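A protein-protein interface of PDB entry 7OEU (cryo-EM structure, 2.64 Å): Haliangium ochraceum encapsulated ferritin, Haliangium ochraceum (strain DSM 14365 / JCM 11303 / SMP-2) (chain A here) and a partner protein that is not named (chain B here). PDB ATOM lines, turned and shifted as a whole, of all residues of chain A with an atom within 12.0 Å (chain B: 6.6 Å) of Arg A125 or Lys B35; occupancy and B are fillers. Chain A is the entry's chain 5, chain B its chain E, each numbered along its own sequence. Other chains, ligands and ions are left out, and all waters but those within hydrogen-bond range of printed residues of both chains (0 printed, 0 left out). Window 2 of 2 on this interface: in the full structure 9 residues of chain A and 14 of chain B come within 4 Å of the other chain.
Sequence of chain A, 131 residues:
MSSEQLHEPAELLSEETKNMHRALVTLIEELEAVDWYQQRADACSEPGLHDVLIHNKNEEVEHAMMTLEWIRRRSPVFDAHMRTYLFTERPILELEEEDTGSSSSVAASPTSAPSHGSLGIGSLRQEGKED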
ATOM      1  N   GLY A 120     -22.222  18.538  28.335  1.00  0.00           N
ATOM      2  CA  GLY A 120     -21.345  18.050  29.384  1.00  0.00           C
ATOM      3  C   GLY A 120     -19.877  18.011  29.022  1.00  0.00           C
ATOM      4  O   GLY A 120     -19.183  17.051  29.376  1.00  0.00           O
ATOM      5  N   ILE A 121     -19.382  19.030  28.325  1.00  0.00           N
ATOM      6  CA  ILE A 121     -17.960  19.092  28.004  1.00  0.00           C
ATOM      7  C   ILE A 121     -17.151  19.486  29.231  1.00  0.00           C
ATOM      8  O   ILE A 121     -16.274  18.742  29.685  1.00  0.00           O
ATOM      9  CB  ILE A 121     -17.707  20.059  26.833  1.00  0.00           C
ATOM     10  CG1 ILE A 121     -18.544  19.674  25.610  1.00  0.00           C
ATOM     11  CG2 ILE A 121     -16.225  20.095  26.490  1.00  0.00           C
ATOM     12  CD1 ILE A 121     -18.583  18.190  25.319  1.00  0.00           C
ATOM     13  N   GLY A 122     -17.434  20.664  29.785  1.00  0.00           N
ATOM     14  CA  GLY A 122     -16.730  21.120  30.966  1.00  0.00           C
ATOM     15  C   GLY A 122     -15.262  21.391  30.689  1.00  0.00           C
ATOM     16  O   GLY A 122     -14.853  21.712  29.569  1.00  0.00           O
ATOM     17  N   SER A 123     -14.455  21.263  31.735  1.00  0.00           N
ATOM     18  CA  SER A 123     -13.019  21.449  31.593  1.00  0.00           C
ATOM     19  C   SER A 123     -12.392  20.266  30.873  1.00  0.00           C
ATOM     20  O   SER A 123     -12.769  19.112  31.089  1.00  0.00           O
ATOM     21  CB  SER A 123     -12.362  21.624  32.959  1.00  0.00           C
ATOM     22  OG  SER A 123     -11.045  22.125  32.823  1.00  0.00           O
ATOM     23  N   LEU A 124     -11.425  20.562  30.008  1.00  0.00           N
ATOM     24  CA  LEU A 124     -10.580  19.544  29.401  1.00  0.00           C
ATOM     25  C   LEU A 124      -9.180  19.542  30.008  1.00  0.00           C
ATOM     26  O   LEU A 124      -8.226  19.104  29.358  1.00  0.00           O
ATOM     27  CB  LEU A 124     -10.517  19.738  27.885  1.00  0.00           C
ATOM     28  CG  LEU A 124     -11.875  19.781  27.178  1.00  0.00           C
ATOM     29  CD1 LEU A 124     -11.709  20.023  25.689  1.00  0.00           C
ATOM     30  CD2 LEU A 124     -12.663  18.505  27.429  1.00  0.00           C
ATOM     31  N   ARG A 125      -9.051  20.032  31.241  1.00  0.00           N
ATOM     32  CA  ARG A 125      -7.777  20.141  31.954  1.00  0.00           C
ATOM     33  C   ARG A 125      -6.787  21.031  31.215  1.00  0.00           C
ATOM     34  O   ARG A 125      -6.547  22.171  31.613  1.00  0.00           O
ATOM     35  CB  ARG A 125      -7.161  18.761  32.190  1.00  0.00           C
ATOM     36  CG  ARG A 125      -7.965  17.864  33.114  1.00  0.00           C
ATOM     37  CD  ARG A 125      -7.286  16.515  33.267  1.00  0.00           C
ATOM     38  NE  ARG A 125      -6.008  16.631  33.963  1.00  0.00           N
ATOM     39  CZ  ARG A 125      -4.825  16.465  33.380  1.00  0.00           C
ATOM     40  NH1 ARG A 125      -4.758  16.178  32.088  1.00  0.00           N
ATOM     41  NH2 ARG A 125      -3.711  16.587  34.086  1.00  0.00           N
ATOM     42  N   PHE B  27     -16.055  18.453  20.060  1.00  0.00           N
ATOM     43  CA  PHE B  27     -15.616  19.382  21.099  1.00  0.00           C
ATOM     44  C   PHE B  27     -14.480  18.796  21.928  1.00  0.00           C
ATOM     45  O   PHE B  27     -13.493  19.482  22.215  1.00  0.00           O
ATOM     46  CB  PHE B  27     -16.791  19.771  21.995  1.00  0.00           C
ATOM     47  CG  PHE B  27     -17.728  20.747  21.358  1.00  0.00           C
ATOM     48  CD1 PHE B  27     -17.240  21.865  20.710  1.00  0.00           C
ATOM     49  CD2 PHE B  27     -19.094  20.546  21.399  1.00  0.00           C
ATOM     50  CE1 PHE B  27     -18.093  22.763  20.118  1.00  0.00           C
ATOM     51  CE2 PHE B  27     -19.950  21.439  20.806  1.00  0.00           C
ATOM     52  CZ  PHE B  27     -19.450  22.550  20.165  1.00  0.00           C
ATOM     53  N   GLN B  28     -14.599  17.529  22.324  1.00  0.00           N
ATOM     54  CA  GLN B  28     -13.519  16.896  23.071  1.00  0.00           C
ATOM     55  C   GLN B  28     -12.253  16.779  22.236  1.00  0.00           C
ATOM     56  O   GLN B  28     -11.148  16.765  22.787  1.00  0.00           O
ATOM     57  CB  GLN B  28     -13.954  15.523  23.574  1.00  0.00           C
ATOM     58  CG  GLN B  28     -15.047  15.570  24.619  1.00  0.00           C
ATOM     59  CD  GLN B  28     -15.463  14.194  25.079  1.00  0.00           C
ATOM     60  OE1 GLN B  28     -14.981  13.186  24.566  1.00  0.00           O
ATOM     61  NE2 GLN B  28     -16.346  14.142  26.062  1.00  0.00           N
ATOM     62  N   GLY B  29     -12.385  16.700  20.912  1.00  0.00           N
ATOM     63  CA  GLY B  29     -11.204  16.630  20.075  1.00  0.00           C
ATOM     64  C   GLY B  29     -10.522  17.957  19.820  1.00  0.00           C
ATOM     65  O   GLY B  29      -9.301  17.997  19.649  1.00  0.00           O
ATOM     66  N   HIS B  30     -11.277  19.058  19.788  1.00  0.00           N
ATOM     67  CA  HIS B  30     -10.746  20.296  19.234  1.00  0.00           C
ATOM     68  C   HIS B  30     -10.687  21.487  20.182  1.00  0.00           C
ATOM     69  O   HIS B  30     -10.104  22.509  19.806  1.00  0.00           O
ATOM     70  CB  HIS B  30     -11.555  20.707  17.995  1.00  0.00           C
ATOM     71  CG  HIS B  30     -11.423  19.756  16.849  1.00  0.00           C
ATOM     72  ND1 HIS B  30     -12.245  18.662  16.691  1.00  0.00           N
ATOM     73  CD2 HIS B  30     -10.567  19.738  15.800  1.00  0.00           C
ATOM     74  CE1 HIS B  30     -11.901  18.008  15.597  1.00  0.00           C
ATOM     75  NE2 HIS B  30     -10.885  18.642  15.037  1.00  0.00           N
ATOM     76  N   LEU B  31     -11.257  21.409  21.380  1.00  0.00           N
ATOM     77  CA  LEU B  31     -11.287  22.569  22.272  1.00  0.00           C
ATOM     78  C   LEU B  31      -9.914  22.736  22.911  1.00  0.00           C
ATOM     79  O   LEU B  31      -9.605  22.110  23.926  1.00  0.00           O
ATOM     80  CB  LEU B  31     -12.375  22.418  23.325  1.00  0.00           C
ATOM     81  CG  LEU B  31     -13.783  22.819  22.886  1.00  0.00           C
ATOM     82  CD1 LEU B  31     -14.800  22.350  23.900  1.00  0.00           C
ATOM     83  CD2 LEU B  31     -13.875  24.318  22.674  1.00  0.00           C
ATOM     84  N   ALA B  32      -9.084  23.594  22.315  1.00  0.00           N
ATOM     85  CA  ALA B  32      -7.708  23.748  22.778  1.00  0.00           C
ATOM     86  C   ALA B  32      -7.635  24.517  24.093  1.00  0.00           C
ATOM     87  O   ALA B  32      -6.915  24.120  25.014  1.00  0.00           O
ATOM     88  CB  ALA B  32      -6.873  24.440  21.706  1.00  0.00           C
ATOM     89  N   GLY B  33      -8.370  25.625  24.197  1.00  0.00           N
ATOM     90  CA  GLY B  33      -8.248  26.472  25.374  1.00  0.00           C
ATOM     91  C   GLY B  33      -8.686  25.786  26.653  1.00  0.00           C
ATOM     92  O   GLY B  33      -8.095  25.996  27.714  1.00  0.00           O
ATOM     93  N   ARG B  34      -9.726  24.953  26.570  1.00  0.00           N
ATOM     94  CA  ARG B  34     -10.279  24.321  27.763  1.00  0.00           C
ATOM     95  C   ARG B  34      -9.302  23.353  28.412  1.00  0.00           C
ATOM     96  O   ARG B  34      -9.394  23.100  29.617  1.00  0.00           O
ATOM     97  CB  ARG B  34     -11.572  23.587  27.417  1.00  0.00           C
ATOM     98  CG  ARG B  34     -12.816  24.366  27.741  1.00  0.00           C
ATOM     99  CD  ARG B  34     -14.026  23.688  27.166  1.00  0.00           C
ATOM    100  NE  ARG B  34     -15.130  24.619  26.993  1.00  0.00           N
ATOM    101  CZ  ARG B  34     -16.334  24.432  27.511  1.00  0.00           C
ATOM    102  NH1 ARG B  34     -16.581  23.348  28.230  1.00  0.00           N
ATOM    103  NH2 ARG B  34     -17.286  25.326  27.309  1.00  0.00           N
ATOM    104  N   LYS B  35      -8.376  22.798  27.642  1.00  0.00           N
ATOM    105  CA  LYS B  35      -7.408  21.852  28.169  1.00  0.00           C
ATOM    106  C   LYS B  35      -6.116  22.526  28.613  1.00  0.00           C
ATOM    107  O   LYS B  35      -5.139  21.837  28.917  1.00  0.00           O
ATOM    108  CB  LYS B  35      -7.143  20.755  27.133  1.00  0.00           C
ATOM    109  CG  LYS B  35      -6.492  21.219  25.856  1.00  0.00           C
ATOM    110  CD  LYS B  35      -6.266  20.057  24.908  1.00  0.00           C
ATOM    111  CE  LYS B  35      -7.590  19.604  24.310  1.00  0.00           C
ATOM    112  NZ  LYS B  35      -7.444  18.551  23.270  1.00  0.00           N
ATOM    113  N   LEU B  36      -6.095  23.857  28.662  1.00  0.00           N
ATOM    114  CA  LEU B  36      -4.943  24.607  29.149  1.00  0.00           C
ATOM    115  C   LEU B  36      -5.282  25.467  30.358  1.00  0.00           C
ATOM    116  O   LEU B  36      -4.623  25.352  31.394  1.00  0.00           O
ATOM    117  CB  LEU B  36      -4.385  25.469  28.014  1.00  0.00           C
ATOM    118  CG  LEU B  36      -3.933  24.682  26.786  1.00  0.00           C
ATOM    119  CD1 LEU B  36      -3.720  25.610  25.609  1.00  0.00           C
ATOM    120  CD2 LEU B  36      -2.666  23.907  27.105  1.00  0.00           C
ATOM    121  N   VAL B  37      -6.301  26.318  30.260  1.00  0.00           N
ATOM    122  CA  VAL B  37      -6.595  27.338  31.263  1.00  0.00           C
ATOM    123  C   VAL B  37      -7.409  26.766  32.416  1.00  0.00           C
ATOM    124  O   VAL B  37      -7.899  25.634  32.348  1.00  0.00           O
ATOM    125  CB  VAL B  37      -7.322  28.532  30.622  1.00  0.00           C
ATOM    126  CG1 VAL B  37      -6.543  29.032  29.427  1.00  0.00           C
ATOM    127  CG2 VAL B  37      -8.733  28.143  30.219  1.00  0.00           C
ATOM    128  N   ASP B  38      -7.540  27.539  33.489  1.00  0.00           N
ATOM    129  CA  ASP B  38      -8.391  27.157  34.606  1.00  0.00           C
ATOM    130  C   ASP B  38      -9.858  27.371  34.245  1.00  0.00           C
ATOM    131  O   ASP B  38     -10.198  28.237  33.438  1.00  0.00           O
ATOM    132  CB  ASP B  38      -8.030  27.966  35.850  1.00  0.00           C
ATOM    133  CG  ASP B  38      -6.533  27.996  36.116  1.00  0.00           C
ATOM    134  OD1 ASP B  38      -5.847  26.991  35.829  1.00  0.00           O
ATOM    135  OD2 ASP B  38      -6.042  29.031  36.607  1.00  0.00           O
ATOM    136  N   PHE B  39     -10.731  26.572  34.855  1.00  0.00           N
ATOM    137  CA  PHE B  39     -12.120  26.459  34.428  1.00  0.00           C
ATOM    138  C   PHE B  39     -13.059  26.744  35.594  1.00  0.00           C
ATOM    139  O   PHE B  39     -12.981  26.084  36.635  1.00  0.00           O
ATOM    140  CB  PHE B  39     -12.381  25.066  33.852  1.00  0.00           C
ATOM    141  CG  PHE B  39     -13.680  24.940  33.115  1.00  0.00           C
ATOM    142  CD1 PHE B  39     -13.754  25.233  31.765  1.00  0.00           C
ATOM    143  CD2 PHE B  39     -14.822  24.505  33.763  1.00  0.00           C
ATOM    144  CE1 PHE B  39     -14.944  25.109  31.080  1.00  0.00           C
ATOM    145  CE2 PHE B  39     -16.015  24.381  33.085  1.00  0.00           C
ATOM    146  CZ  PHE B  39     -16.076  24.682  31.741  1.00  0.00           C
ATOM    147  N   PRO B 202       2.040  19.407  28.735  1.00  0.00           N
ATOM    148  CA  PRO B 202       1.324  18.902  27.563  1.00  0.00           C
ATOM    149  C   PRO B 202       1.683  19.673  26.302  1.00  0.00           C
ATOM    150  O   PRO B 202       2.115  20.825  26.337  1.00  0.00           O
ATOM    151  CB  PRO B 202      -0.147  19.113  27.937  1.00  0.00           C
ATOM    152  CG  PRO B 202      -0.119  20.291  28.840  1.00  0.00           C
ATOM    153  CD  PRO B 202       1.156  20.170  29.634  1.00  0.00           C
ATOM    154  N   VAL B 204      -0.263  20.646  22.808  1.00  0.00           N
ATOM    155  CA  VAL B 204      -1.638  20.688  22.330  1.00  0.00           C
ATOM    156  C   VAL B 204      -1.696  21.427  21.003  1.00  0.00           C
ATOM    157  O   VAL B 204      -0.912  22.350  20.754  1.00  0.00           O
ATOM    158  CB  VAL B 204      -2.581  21.347  23.359  1.00  0.00           C
ATOM    159  CG1 VAL B 204      -2.575  20.563  24.657  1.00  0.00           C
ATOM    160  CG2 VAL B 204      -2.181  22.785  23.605  1.00  0.00           C
ATOM    161  N   ARG B 205      -2.622  21.006  20.151  1.00  0.00           N
ATOM    162  CA  ARG B 205      -2.875  21.641  18.866  1.00  0.00           C
ATOM    163  C   ARG B 205      -4.045  22.606  19.003  1.00  0.00           C
ATOM    164  O   ARG B 205      -5.110  22.230  19.500  1.00  0.00           O
ATOM    165  CB  ARG B 205      -3.178  20.589  17.799  1.00  0.00           C
ATOM    166  CG  ARG B 205      -3.441  21.150  16.416  1.00  0.00           C
ATOM    167  CD  ARG B 205      -3.446  20.046  15.371  1.00  0.00           C
ATOM    168  NE  ARG B 205      -4.453  20.289  14.343  1.00  0.00           N
ATOM    169  CZ  ARG B 205      -4.269  21.065  13.284  1.00  0.00           C
ATOM    170  NH1 ARG B 205      -3.104  21.665  13.098  1.00  0.00           N
ATOM    171  NH2 ARG B 205      -5.244  21.238  12.403  1.00  0.00           N
ATOM    172  N   MET B 217       1.552  25.942  32.981  1.00  0.00           N
ATOM    173  CA  MET B 217       0.423  25.191  33.513  1.00  0.00           C
ATOM    174  C   MET B 217       0.352  25.268  35.030  1.00  0.00           C
ATOM    175  O   MET B 217      -0.199  24.366  35.667  1.00  0.00           O
ATOM    176  CB  MET B 217       0.495  23.730  33.071  1.00  0.00           C
ATOM    177  CG  MET B 217       0.344  23.488  31.582  1.00  0.00           C
ATOM    178  SD  MET B 217      -1.246  24.021  30.927  1.00  0.00           S
ATOM    179  CE  MET B 217      -0.788  25.562  30.144  1.00  0.00           C
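Of the 17 printed residues of chain B, 7 touch a printed residue of chain A. Hydrophobic or aromatic side chains of chain B that line the printed part of chain A: Leu B31 and Phe B39. Of the 6 printed residues of chain A, 5 touch a printed residue of chain B. Printed residues of chain A that touch a printed residue of chain B: Ile A121, Gly A122, Ser A123, Leu A124 and Arg A125. Hydrophobic or aromatic side chains of chain A within 4 Å of the printed part of chain B: Ile A121 and Leu A124. Among the printed residues, 14 pairs touch across the chains.
The side-chain hydroxyl (OG) of Ser A123 is in hydrogen-bond range of the backbone NH (N) of Arg A125 (3.3 Å).
Of the printed residues of chain B, Ser A123 touches Arg B34 (3.7 Å) and Phe B39 (3.4 Å). Arg A125 touches just these residues of chain B: Arg B34, Lys B35, Leu B36 and Val B37. No residue of chain A comes within 4 Å of Gly B29. Leu B31 touches just these residues of chain A: Ile A121 and Leu A124. Ala B32 touches none of the printed residues of chain A. No residue of chain A comes within 4 Å of Gly B33. Of the printed residues of chain A, Arg B34 touches Ile A121, Gly A122, Ser A123, Leu A124 and Arg A125. Of chain A, only Leu A124 and Arg A125 come within 4 Å of Lys B35. Leu B36 touches one residue of chain A. Val B37 touches just one residue of chain A: Arg A125. No residue of chain A comes within 4 Å of Pro B202. No residue of chain A comes within 4 Å of Val B204. The nearest residue of chain A that does not touch Lys B35 is Ser A123 (5.7 Å).
NH1 of Arg B34 lies within hydrogen-bond range of O of Gly A122, 2.7 Å away. The backbone carbonyl oxygen of Arg B34 lies within hydrogen-bond range of the backbone NH of Leu A124 (3.3 Å). O of Arg A125 sits at hydrogen-bond distance from N of Leu B36, 3.4 Å away. The backbone carbonyl oxygen (O) of Arg B34 lies within hydrogen-bond range of the backbone NH (N) of Arg A125, at 3.5 Å. O of Lys B35 sits close to O of Arg A125 (3.1 Å).
Among the printed residues, merely in contact across the chains: Ile A121 with Leu B31 (3.7 Å), Ile A121 with Arg B34 (3.7 Å), Gly A122 with Phe B39 (3.5 Å), Ser A123 with Arg B34 (3.7 Å), Ser A123 with Phe B39 (3.4 Å), Leu A124 with Phe B27 (3.9 Å), Leu A124 with Leu B31 (3.4 Å), Leu A124 with Lys B35 (3.0 Å) and Arg A125 with Val B37 (3.8 Å).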
